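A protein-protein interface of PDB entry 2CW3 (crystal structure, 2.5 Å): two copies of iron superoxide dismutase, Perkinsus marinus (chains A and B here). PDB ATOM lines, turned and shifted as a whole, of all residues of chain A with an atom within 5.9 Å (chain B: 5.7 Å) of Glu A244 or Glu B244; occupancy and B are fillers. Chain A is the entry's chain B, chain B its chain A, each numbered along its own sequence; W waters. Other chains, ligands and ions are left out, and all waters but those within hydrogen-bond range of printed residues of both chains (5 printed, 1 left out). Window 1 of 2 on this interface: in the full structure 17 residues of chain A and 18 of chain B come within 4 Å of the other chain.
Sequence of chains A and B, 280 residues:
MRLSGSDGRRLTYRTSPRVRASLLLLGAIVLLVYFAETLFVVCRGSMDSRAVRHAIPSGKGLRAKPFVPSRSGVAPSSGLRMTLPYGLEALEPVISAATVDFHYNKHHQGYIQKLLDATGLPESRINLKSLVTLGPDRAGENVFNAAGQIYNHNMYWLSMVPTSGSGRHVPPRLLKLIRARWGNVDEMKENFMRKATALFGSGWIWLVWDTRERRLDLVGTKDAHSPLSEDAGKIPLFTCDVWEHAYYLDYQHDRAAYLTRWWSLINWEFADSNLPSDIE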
ATOM      1  N   HIS A 107     -23.245  20.529  -0.022  1.00  0.00           N
ATOM      2  CA  HIS A 107     -23.127  21.980  -0.215  1.00  0.00           C
ATOM      3  C   HIS A 107     -23.612  22.376  -1.580  1.00  0.00           C
ATOM      4  O   HIS A 107     -24.666  23.004  -1.697  1.00  0.00           O
ATOM      5  CB  HIS A 107     -21.700  22.505   0.017  1.00  0.00           C
ATOM      6  CG  HIS A 107     -21.323  22.581   1.462  1.00  0.00           C
ATOM      7  ND1 HIS A 107     -20.692  21.546   2.120  1.00  0.00           N
ATOM      8  CD2 HIS A 107     -21.540  23.540   2.389  1.00  0.00           C
ATOM      9  CE1 HIS A 107     -20.515  21.875   3.385  1.00  0.00           C
ATOM     10  NE2 HIS A 107     -21.007  23.086   3.570  1.00  0.00           N
ATOM     11  N   SER A 202     -15.877  33.949   4.715  1.00  0.00           N
ATOM     12  CA  SER A 202     -16.237  33.142   3.527  1.00  0.00           C
ATOM     13  C   SER A 202     -16.062  33.937   2.239  1.00  0.00           C
ATOM     14  O   SER A 202     -16.371  35.124   2.181  1.00  0.00           O
ATOM     15  CB  SER A 202     -17.686  32.636   3.621  1.00  0.00           C
ATOM     16  OG  SER A 202     -17.941  32.030   4.881  1.00  0.00           O
ATOM     17  N   VAL A 242     -12.851  29.416  -1.186  1.00  0.00           N
ATOM     18  CA  VAL A 242     -12.097  29.685   0.038  1.00  0.00           C
ATOM     19  C   VAL A 242     -12.938  29.603   1.355  1.00  0.00           C
ATOM     20  O   VAL A 242     -12.436  29.878   2.457  1.00  0.00           O
ATOM     21  CB  VAL A 242     -11.227  30.980  -0.171  1.00  0.00           C
ATOM     22  CG1 VAL A 242     -11.215  31.896   1.039  1.00  0.00           C
ATOM     23  CG2 VAL A 242      -9.807  30.606  -0.640  1.00  0.00           C
ATOM     24  N   TRP A 243     -14.207  29.194   1.229  1.00  0.00           N
ATOM     25  CA  TRP A 243     -15.040  28.860   2.391  1.00  0.00           C
ATOM     26  C   TRP A 243     -14.359  27.727   3.142  1.00  0.00           C
ATOM     27  O   TRP A 243     -13.743  26.848   2.527  1.00  0.00           O
ATOM     28  CB  TRP A 243     -16.416  28.345   1.959  1.00  0.00           C
ATOM     29  CG  TRP A 243     -17.365  29.381   1.488  1.00  0.00           C
ATOM     30  CD1 TRP A 243     -17.160  30.281   0.488  1.00  0.00           C
ATOM     31  CD2 TRP A 243     -18.705  29.599   1.972  1.00  0.00           C
ATOM     32  NE1 TRP A 243     -18.276  31.068   0.340  1.00  0.00           N
ATOM     33  CE2 TRP A 243     -19.244  30.665   1.226  1.00  0.00           C
ATOM     34  CE3 TRP A 243     -19.490  29.005   2.976  1.00  0.00           C
ATOM     35  CZ2 TRP A 243     -20.543  31.162   1.446  1.00  0.00           C
ATOM     36  CZ3 TRP A 243     -20.785  29.488   3.192  1.00  0.00           C
ATOM     37  CH2 TRP A 243     -21.293  30.566   2.436  1.00  0.00           C
ATOM     38  N   GLU A 244     -14.492  27.711   4.460  1.00  0.00           N
ATOM     39  CA  GLU A 244     -13.813  26.690   5.225  1.00  0.00           C
ATOM     40  C   GLU A 244     -14.296  25.263   4.887  1.00  0.00           C
ATOM     41  O   GLU A 244     -13.535  24.302   5.034  1.00  0.00           O
ATOM     42  CB  GLU A 244     -13.917  26.980   6.713  1.00  0.00           C
ATOM     43  CG  GLU A 244     -13.353  28.301   7.143  1.00  0.00           C
ATOM     44  CD  GLU A 244     -13.610  28.585   8.620  1.00  0.00           C
ATOM     45  OE1 GLU A 244     -12.641  28.933   9.305  1.00  0.00           O
ATOM     46  OE2 GLU A 244     -14.762  28.462   9.119  1.00  0.00           O
ATOM     47  N   HIS A 245     -15.540  25.119   4.419  1.00  0.00           N
ATOM     48  CA  HIS A 245     -16.039  23.799   4.031  1.00  0.00           C
ATOM     49  C   HIS A 245     -15.153  23.227   2.924  1.00  0.00           C
ATOM     50  O   HIS A 245     -15.044  22.015   2.776  1.00  0.00           O
ATOM     51  CB  HIS A 245     -17.555  23.799   3.657  1.00  0.00           C
ATOM     52  CG  HIS A 245     -17.915  24.551   2.398  1.00  0.00           C
ATOM     53  ND1 HIS A 245     -19.009  25.388   2.323  1.00  0.00           N
ATOM     54  CD2 HIS A 245     -17.351  24.573   1.161  1.00  0.00           C
ATOM     55  CE1 HIS A 245     -19.096  25.901   1.108  1.00  0.00           C
ATOM     56  NE2 HIS A 245     -18.095  25.433   0.381  1.00  0.00           N
ATOM     57  N   ALA A 246     -14.501  24.115   2.164  1.00  0.00           N
ATOM     58  CA  ALA A 246     -13.656  23.688   1.048  1.00  0.00           C
ATOM     59  C   ALA A 246     -12.435  22.949   1.515  1.00  0.00           C
ATOM     60  O   ALA A 246     -11.909  22.122   0.778  1.00  0.00           O
ATOM     61  CB  ALA A 246     -13.250  24.848   0.174  1.00  0.00           C
ATOM     62  N   TYR A 247     -11.966  23.234   2.728  1.00  0.00           N
ATOM     63  CA  TYR A 247     -10.669  22.665   3.148  1.00  0.00           C
ATOM     64  C   TYR A 247     -10.606  22.114   4.567  1.00  0.00           C
ATOM     65  O   TYR A 247      -9.590  21.510   4.943  1.00  0.00           O
ATOM     66  CB  TYR A 247      -9.521  23.676   2.930  1.00  0.00           C
ATOM     67  CG  TYR A 247      -9.682  24.984   3.676  1.00  0.00           C
ATOM     68  CD1 TYR A 247      -9.293  25.104   5.015  1.00  0.00           C
ATOM     69  CD2 TYR A 247     -10.247  26.105   3.052  1.00  0.00           C
ATOM     70  CE1 TYR A 247      -9.449  26.324   5.711  1.00  0.00           C
ATOM     71  CE2 TYR A 247     -10.428  27.317   3.744  1.00  0.00           C
ATOM     72  CZ  TYR A 247     -10.026  27.413   5.062  1.00  0.00           C
ATOM     73  OH  TYR A 247     -10.203  28.595   5.746  1.00  0.00           O
ATOM     74  N   TYR A 248     -11.666  22.308   5.351  1.00  0.00           N
ATOM     75  CA  TYR A 248     -11.554  22.082   6.797  1.00  0.00           C
ATOM     76  C   TYR A 248     -11.263  20.653   7.236  1.00  0.00           C
ATOM     77  O   TYR A 248     -10.514  20.447   8.187  1.00  0.00           O
ATOM     78  CB  TYR A 248     -12.720  22.680   7.617  1.00  0.00           C
ATOM     79  CG  TYR A 248     -12.211  23.109   8.970  1.00  0.00           C
ATOM     80  CD1 TYR A 248     -11.492  24.300   9.117  1.00  0.00           C
ATOM     81  CD2 TYR A 248     -12.379  22.308  10.073  1.00  0.00           C
ATOM     82  CE1 TYR A 248     -10.986  24.699  10.361  1.00  0.00           C
ATOM     83  CE2 TYR A 248     -11.873  22.676  11.316  1.00  0.00           C
ATOM     84  CZ  TYR A 248     -11.166  23.868  11.464  1.00  0.00           C
ATOM     85  OH  TYR A 248     -10.661  24.229  12.714  1.00  0.00           O
ATOM     86  N   LEU A 249     -11.846  19.678   6.549  1.00  0.00           N
ATOM     87  CA  LEU A 249     -11.629  18.274   6.883  1.00  0.00           C
ATOM     88  C   LEU A 249     -10.224  17.784   6.579  1.00  0.00           C
ATOM     89  O   LEU A 249      -9.789  16.773   7.117  1.00  0.00           O
ATOM     90  CB  LEU A 249     -12.623  17.395   6.134  1.00  0.00           C
ATOM     91  CG  LEU A 249     -14.073  17.684   6.495  1.00  0.00           C
ATOM     92  CD1 LEU A 249     -15.023  16.891   5.580  1.00  0.00           C
ATOM     93  CD2 LEU A 249     -14.278  17.357   7.947  1.00  0.00           C
ATOM     94  N   ARG A 255      -5.263  27.322   5.881  1.00  0.00           N
ATOM     95  CA  ARG A 255      -5.747  27.579   4.534  1.00  0.00           C
ATOM     96  C   ARG A 255      -4.601  27.639   3.516  1.00  0.00           C
ATOM     97  O   ARG A 255      -4.700  27.079   2.424  1.00  0.00           O
ATOM     98  CB  ARG A 255      -6.585  28.853   4.471  1.00  0.00           C
ATOM     99  CG  ARG A 255      -7.235  29.047   3.121  1.00  0.00           C
ATOM    100  CD  ARG A 255      -7.735  30.429   2.911  1.00  0.00           C
ATOM    101  NE  ARG A 255      -8.901  30.733   3.723  1.00  0.00           N
ATOM    102  CZ  ARG A 255      -9.403  31.960   3.868  1.00  0.00           C
ATOM    103  NH1 ARG A 255      -8.849  32.999   3.238  1.00  0.00           N
ATOM    104  NH2 ARG A 255     -10.470  32.149   4.639  1.00  0.00           N
ATOM    105  N   HIS B 107      -7.370  28.605  15.848  1.00  0.00           N
ATOM    106  CA  HIS B 107      -8.092  29.827  15.483  1.00  0.00           C
ATOM    107  C   HIS B 107      -7.941  30.930  16.537  1.00  0.00           C
ATOM    108  O   HIS B 107      -7.369  31.983  16.249  1.00  0.00           O
ATOM    109  CB  HIS B 107      -9.559  29.554  15.198  1.00  0.00           C
ATOM    110  CG  HIS B 107      -9.784  28.664  14.022  1.00  0.00           C
ATOM    111  ND1 HIS B 107      -9.662  29.104  12.722  1.00  0.00           N
ATOM    112  CD2 HIS B 107     -10.129  27.360  13.946  1.00  0.00           C
ATOM    113  CE1 HIS B 107      -9.920  28.110  11.895  1.00  0.00           C
ATOM    114  NE2 HIS B 107     -10.196  27.037  12.612  1.00  0.00           N
ATOM    115  N   SER B 202     -19.941  33.454   7.065  1.00  0.00           N
ATOM    116  CA  SER B 202     -19.284  33.385   8.367  1.00  0.00           C
ATOM    117  C   SER B 202     -19.885  34.448   9.274  1.00  0.00           C
ATOM    118  O   SER B 202     -19.917  35.641   8.913  1.00  0.00           O
ATOM    119  CB  SER B 202     -17.786  33.618   8.203  1.00  0.00           C
ATOM    120  OG  SER B 202     -17.219  32.660   7.324  1.00  0.00           O
ATOM    121  N   VAL B 242     -20.988  30.716  14.455  1.00  0.00           N
ATOM    122  CA  VAL B 242     -21.557  30.056  13.297  1.00  0.00           C
ATOM    123  C   VAL B 242     -20.565  29.915  12.102  1.00  0.00           C
ATOM    124  O   VAL B 242     -20.946  29.502  10.992  1.00  0.00           O
ATOM    125  CB  VAL B 242     -22.941  30.679  12.957  1.00  0.00           C
ATOM    126  CG1 VAL B 242     -23.251  30.602  11.495  1.00  0.00           C
ATOM    127  CG2 VAL B 242     -24.010  29.980  13.736  1.00  0.00           C
ATOM    128  N   TRP B 243     -19.301  30.268  12.329  1.00  0.00           N
ATOM    129  CA  TRP B 243     -18.254  30.010  11.343  1.00  0.00           C
ATOM    130  C   TRP B 243     -18.163  28.509  11.190  1.00  0.00           C
ATOM    131  O   TRP B 243     -18.300  27.777  12.174  1.00  0.00           O
ATOM    132  CB  TRP B 243     -16.904  30.532  11.828  1.00  0.00           C
ATOM    133  CG  TRP B 243     -16.695  32.015  11.665  1.00  0.00           C
ATOM    134  CD1 TRP B 243     -17.458  33.020  12.193  1.00  0.00           C
ATOM    135  CD2 TRP B 243     -15.630  32.652  10.953  1.00  0.00           C
ATOM    136  NE1 TRP B 243     -16.933  34.244  11.856  1.00  0.00           N
ATOM    137  CE2 TRP B 243     -15.812  34.049  11.091  1.00  0.00           C
ATOM    138  CE3 TRP B 243     -14.537  32.180  10.214  1.00  0.00           C
ATOM    139  CZ2 TRP B 243     -14.956  34.977  10.503  1.00  0.00           C
ATOM    140  CZ3 TRP B 243     -13.677  33.095   9.645  1.00  0.00           C
ATOM    141  CH2 TRP B 243     -13.888  34.483   9.785  1.00  0.00           C
ATOM    142  N   GLU B 244     -17.945  28.042   9.965  1.00  0.00           N
ATOM    143  CA  GLU B 244     -17.886  26.613   9.718  1.00  0.00           C
ATOM    144  C   GLU B 244     -16.836  25.919  10.569  1.00  0.00           C
ATOM    145  O   GLU B 244     -17.008  24.761  10.922  1.00  0.00           O
ATOM    146  CB  GLU B 244     -17.669  26.312   8.235  1.00  0.00           C
ATOM    147  CG  GLU B 244     -18.907  26.554   7.366  1.00  0.00           C
ATOM    148  CD  GLU B 244     -18.592  26.478   5.886  1.00  0.00           C
ATOM    149  OE1 GLU B 244     -19.446  26.028   5.099  1.00  0.00           O
ATOM    150  OE2 GLU B 244     -17.469  26.854   5.503  1.00  0.00           O
ATOM    151  N   HIS B 245     -15.749  26.614  10.914  1.00  0.00           N
ATOM    152  CA  HIS B 245     -14.725  25.990  11.768  1.00  0.00           C
ATOM    153  C   HIS B 245     -15.269  25.588  13.152  1.00  0.00           C
ATOM    154  O   HIS B 245     -14.740  24.681  13.809  1.00  0.00           O
ATOM    155  CB  HIS B 245     -13.442  26.830  11.875  1.00  0.00           C
ATOM    156  CG  HIS B 245     -13.603  28.135  12.604  1.00  0.00           C
ATOM    157  ND1 HIS B 245     -13.233  29.341  12.055  1.00  0.00           N
ATOM    158  CD2 HIS B 245     -14.080  28.421  13.839  1.00  0.00           C
ATOM    159  CE1 HIS B 245     -13.482  30.314  12.912  1.00  0.00           C
ATOM    160  NE2 HIS B 245     -14.006  29.784  14.002  1.00  0.00           N
ATOM    161  N   ALA B 246     -16.340  26.247  13.595  1.00  0.00           N
ATOM    162  CA  ALA B 246     -16.905  25.912  14.891  1.00  0.00           C
ATOM    163  C   ALA B 246     -17.534  24.505  14.929  1.00  0.00           C
ATOM    164  O   ALA B 246     -17.541  23.878  15.968  1.00  0.00           O
ATOM    165  CB  ALA B 246     -17.862  26.961  15.334  1.00  0.00           C
ATOM    166  N   TYR B 247     -18.019  23.992  13.796  1.00  0.00           N
ATOM    167  CA  TYR B 247     -18.739  22.697  13.786  1.00  0.00           C
ATOM    168  C   TYR B 247     -18.356  21.680  12.721  1.00  0.00           C
ATOM    169  O   TYR B 247     -18.837  20.546  12.775  1.00  0.00           O
ATOM    170  CB  TYR B 247     -20.255  22.920  13.666  1.00  0.00           C
ATOM    171  CG  TYR B 247     -20.686  23.736  12.461  1.00  0.00           C
ATOM    172  CD1 TYR B 247     -20.909  23.133  11.222  1.00  0.00           C
ATOM    173  CD2 TYR B 247     -20.900  25.106  12.570  1.00  0.00           C
ATOM    174  CE1 TYR B 247     -21.318  23.890  10.116  1.00  0.00           C
ATOM    175  CE2 TYR B 247     -21.308  25.873  11.477  1.00  0.00           C
ATOM    176  CZ  TYR B 247     -21.512  25.265  10.262  1.00  0.00           C
ATOM    177  OH  TYR B 247     -21.913  26.018   9.191  1.00  0.00           O
ATOM    178  N   TYR B 248     -17.524  22.077  11.764  1.00  0.00           N
ATOM    179  CA  TYR B 248     -17.345  21.288  10.538  1.00  0.00           C
ATOM    180  C   TYR B 248     -16.718  19.903  10.742  1.00  0.00           C
ATOM    181  O   TYR B 248     -17.148  18.915  10.143  1.00  0.00           O
ATOM    182  CB  TYR B 248     -16.575  22.052   9.454  1.00  0.00           C
ATOM    183  CG  TYR B 248     -17.044  21.596   8.116  1.00  0.00           C
ATOM    184  CD1 TYR B 248     -18.239  22.083   7.579  1.00  0.00           C
ATOM    185  CD2 TYR B 248     -16.362  20.608   7.413  1.00  0.00           C
ATOM    186  CE1 TYR B 248     -18.709  21.631   6.352  1.00  0.00           C
ATOM    187  CE2 TYR B 248     -16.833  20.150   6.179  1.00  0.00           C
ATOM    188  CZ  TYR B 248     -17.998  20.672   5.658  1.00  0.00           C
ATOM    189  OH  TYR B 248     -18.467  20.225   4.445  1.00  0.00           O
ATOM    190  N   LEU B 249     -15.688  19.848  11.573  1.00  0.00           N
ATOM    191  CA  LEU B 249     -15.140  18.580  11.993  1.00  0.00           C
ATOM    192  C   LEU B 249     -16.226  17.641  12.535  1.00  0.00           C
ATOM    193  O   LEU B 249     -16.197  16.440  12.259  1.00  0.00           O
ATOM    194  CB  LEU B 249     -14.094  18.823  13.075  1.00  0.00           C
ATOM    195  CG  LEU B 249     -12.611  18.731  12.724  1.00  0.00           C
ATOM    196  CD1 LEU B 249     -12.255  19.109  11.264  1.00  0.00           C
ATOM    197  CD2 LEU B 249     -11.827  19.537  13.751  1.00  0.00           C
ATOM    198  N   ARG B 255     -25.286  22.320   9.963  1.00  0.00           N
ATOM    199  CA  ARG B 255     -25.242  23.376  10.972  1.00  0.00           C
ATOM    200  C   ARG B 255     -26.411  23.253  11.983  1.00  0.00           C
ATOM    201  O   ARG B 255     -26.252  23.534  13.166  1.00  0.00           O
ATOM    202  CB  ARG B 255     -25.236  24.762  10.294  1.00  0.00           C
ATOM    203  CG  ARG B 255     -24.907  25.888  11.241  1.00  0.00           C
ATOM    204  CD  ARG B 255     -25.304  27.226  10.698  1.00  0.00           C
ATOM    205  NE  ARG B 255     -24.363  27.767   9.706  1.00  0.00           N
ATOM    206  CZ  ARG B 255     -24.562  28.900   9.040  1.00  0.00           C
ATOM    207  NH1 ARG B 255     -25.658  29.612   9.251  1.00  0.00           N
ATOM    208  NH2 ARG B 255     -23.680  29.319   8.156  1.00  0.00           N
HETATM  209  O   HOH W   1     -16.792  29.977   8.244  1.00  0.00           O
HETATM  210  O   HOH W   2     -12.099  24.521  14.916  1.00  0.00           O
HETATM  211  O   HOH W   3     -16.935  29.614   5.461  1.00  0.00           O
HETATM  212  O   HOH W   4     -16.771  20.096   2.033  1.00  0.00           O
HETATM  213  O   HOH W   5     -18.134  35.422   5.303  1.00  0.00           O
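Ser A202 touches its own counterpart, Ser B202.
Glu A244 touches its own counterpart, Glu B244.
His A245 touches Tyr B248, and with the chains exchanged Tyr A248 touches His B245.
Tyr A248 touches Leu B249, and with the chains exchanged Leu A249 touches Tyr B248.
Positions printed for both chains: 107, 202, 242, 243, 244, 245, 246, 247, 248, 249 and 255.
Of the 14 pairs that touch across the chains among the printed residues, 14 have their exchanged pair printed and touching as well.
His A107 touches Glu B244 (NE2 to OE1, 3.7 Å).
Trp A243 touches Glu B244.
His B107 touches Glu A244 (CE1 to OE1, 3.8 Å).
Trp B243 touches Glu A244 (CE3 to OE1, 3.9 Å).
CB of His A245 touches CE1 of Tyr B248, 3.6 Å away.
CE1 of Tyr A248 touches CB of His B245 (3.6 Å).
Tyr A248 touches Leu B249 (CD2 to CD1, 3.4 Å).
Tyr B248 touches Leu A249 (CE2 to CG, 3.7 Å).
Of the 11 printed residues of chain A, 7 touch a printed residue of chain B.
Hydrophobic or aromatic side chains of chain A that line the printed part of chain B: His A107, Trp A243, His A245, Tyr A248 and Leu A249.
Of the 11 printed residues of chain B, 7 touch a printed residue of chain A.
Printed residues of chain B that touch a printed residue of chain A: His B107, Ser B202, Trp B243, Glu B244, His B245, Tyr B248 and Leu B249.
Hydrophobic or aromatic side chains of chain B that line the printed part of chain A: His B107, Trp B243, His B245, Tyr B248 and Leu B249.
Along chain B the printed residues that touch a printed residue of chain A span positions 107 to 249.
Among the printed residues, 14 pairs touch across the chains.
Among the printed residues, no Asp or Glu carboxylate lies within 4 Å of a Lys or Arg side-chain nitrogen of the other chain.
Water W2 bridges OH of Tyr A248 and O of His B245.
Water W1 lies within hydrogen-bond range of OE2 of Glu A244 (2.7 Å), N of Glu B244 (2.8 Å) and OG of Ser B202 (2.9 Å).
Water W3 lies within hydrogen-bond range of the side-chain hydroxyl (OG) of Ser A202, the side-chain carboxylate (OE2) of Glu B244 and the backbone NH (N) of Glu A244.
Water W4 bridges the backbone carbonyl oxygen (O) of His A245 (2.7 Å) and the side-chain hydroxyl (OH) of Tyr B248 (3.0 Å).
Water W5 bridges the backbone NH of Ser A202 (2.8 Å) and the backbone NH of Ser B202 (3.2 Å).
A ring nitrogen (ND1) of His A245 sits close to a ring nitrogen (NE2) of His A107.
NE2 of His B107 sits at hydrogen-bond distance from OH of Tyr A248.
OH of Tyr B248 sits close to ND1 of His A107, at 3.5 Å.
The side-chain carboxylate (OE2) of Glu B244 sits at hydrogen-bond distance from the backbone NH (N) of Glu A244 (3.3 Å).
The side-chain carboxylate (OE2) of Glu B244 lies within hydrogen-bond range of the backbone NH (N) of His A245 (2.8 Å).
OG of Ser B202 sits at hydrogen-bond distance from OG of Ser A202, 2.6 Å away.
The backbone NH (N) of His B245 lies within hydrogen-bond range of the side-chain carboxylate (OE2) of Glu A244, at 2.8 Å.
Printed residues of chain B within 4 Å of Glu A244: His B107, Trp B243, Glu B244 and His B245.
Of the printed residues of chain B, His A245 touches Glu B244 (2.8 Å) and Tyr B248 (3.6 Å).
Tyr A247 touches none of the printed residues of chain B.
Of the printed residues of chain A, His B107 touches Glu A244 and Tyr A248.
Of the printed residues of chain A, Trp B243 touches Glu A244 (3.9 Å).
Glu B244 touches four residues of chain A.
The nearest residue of chain B that does not touch Glu A244 is Ser B202 (5.2 Å).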
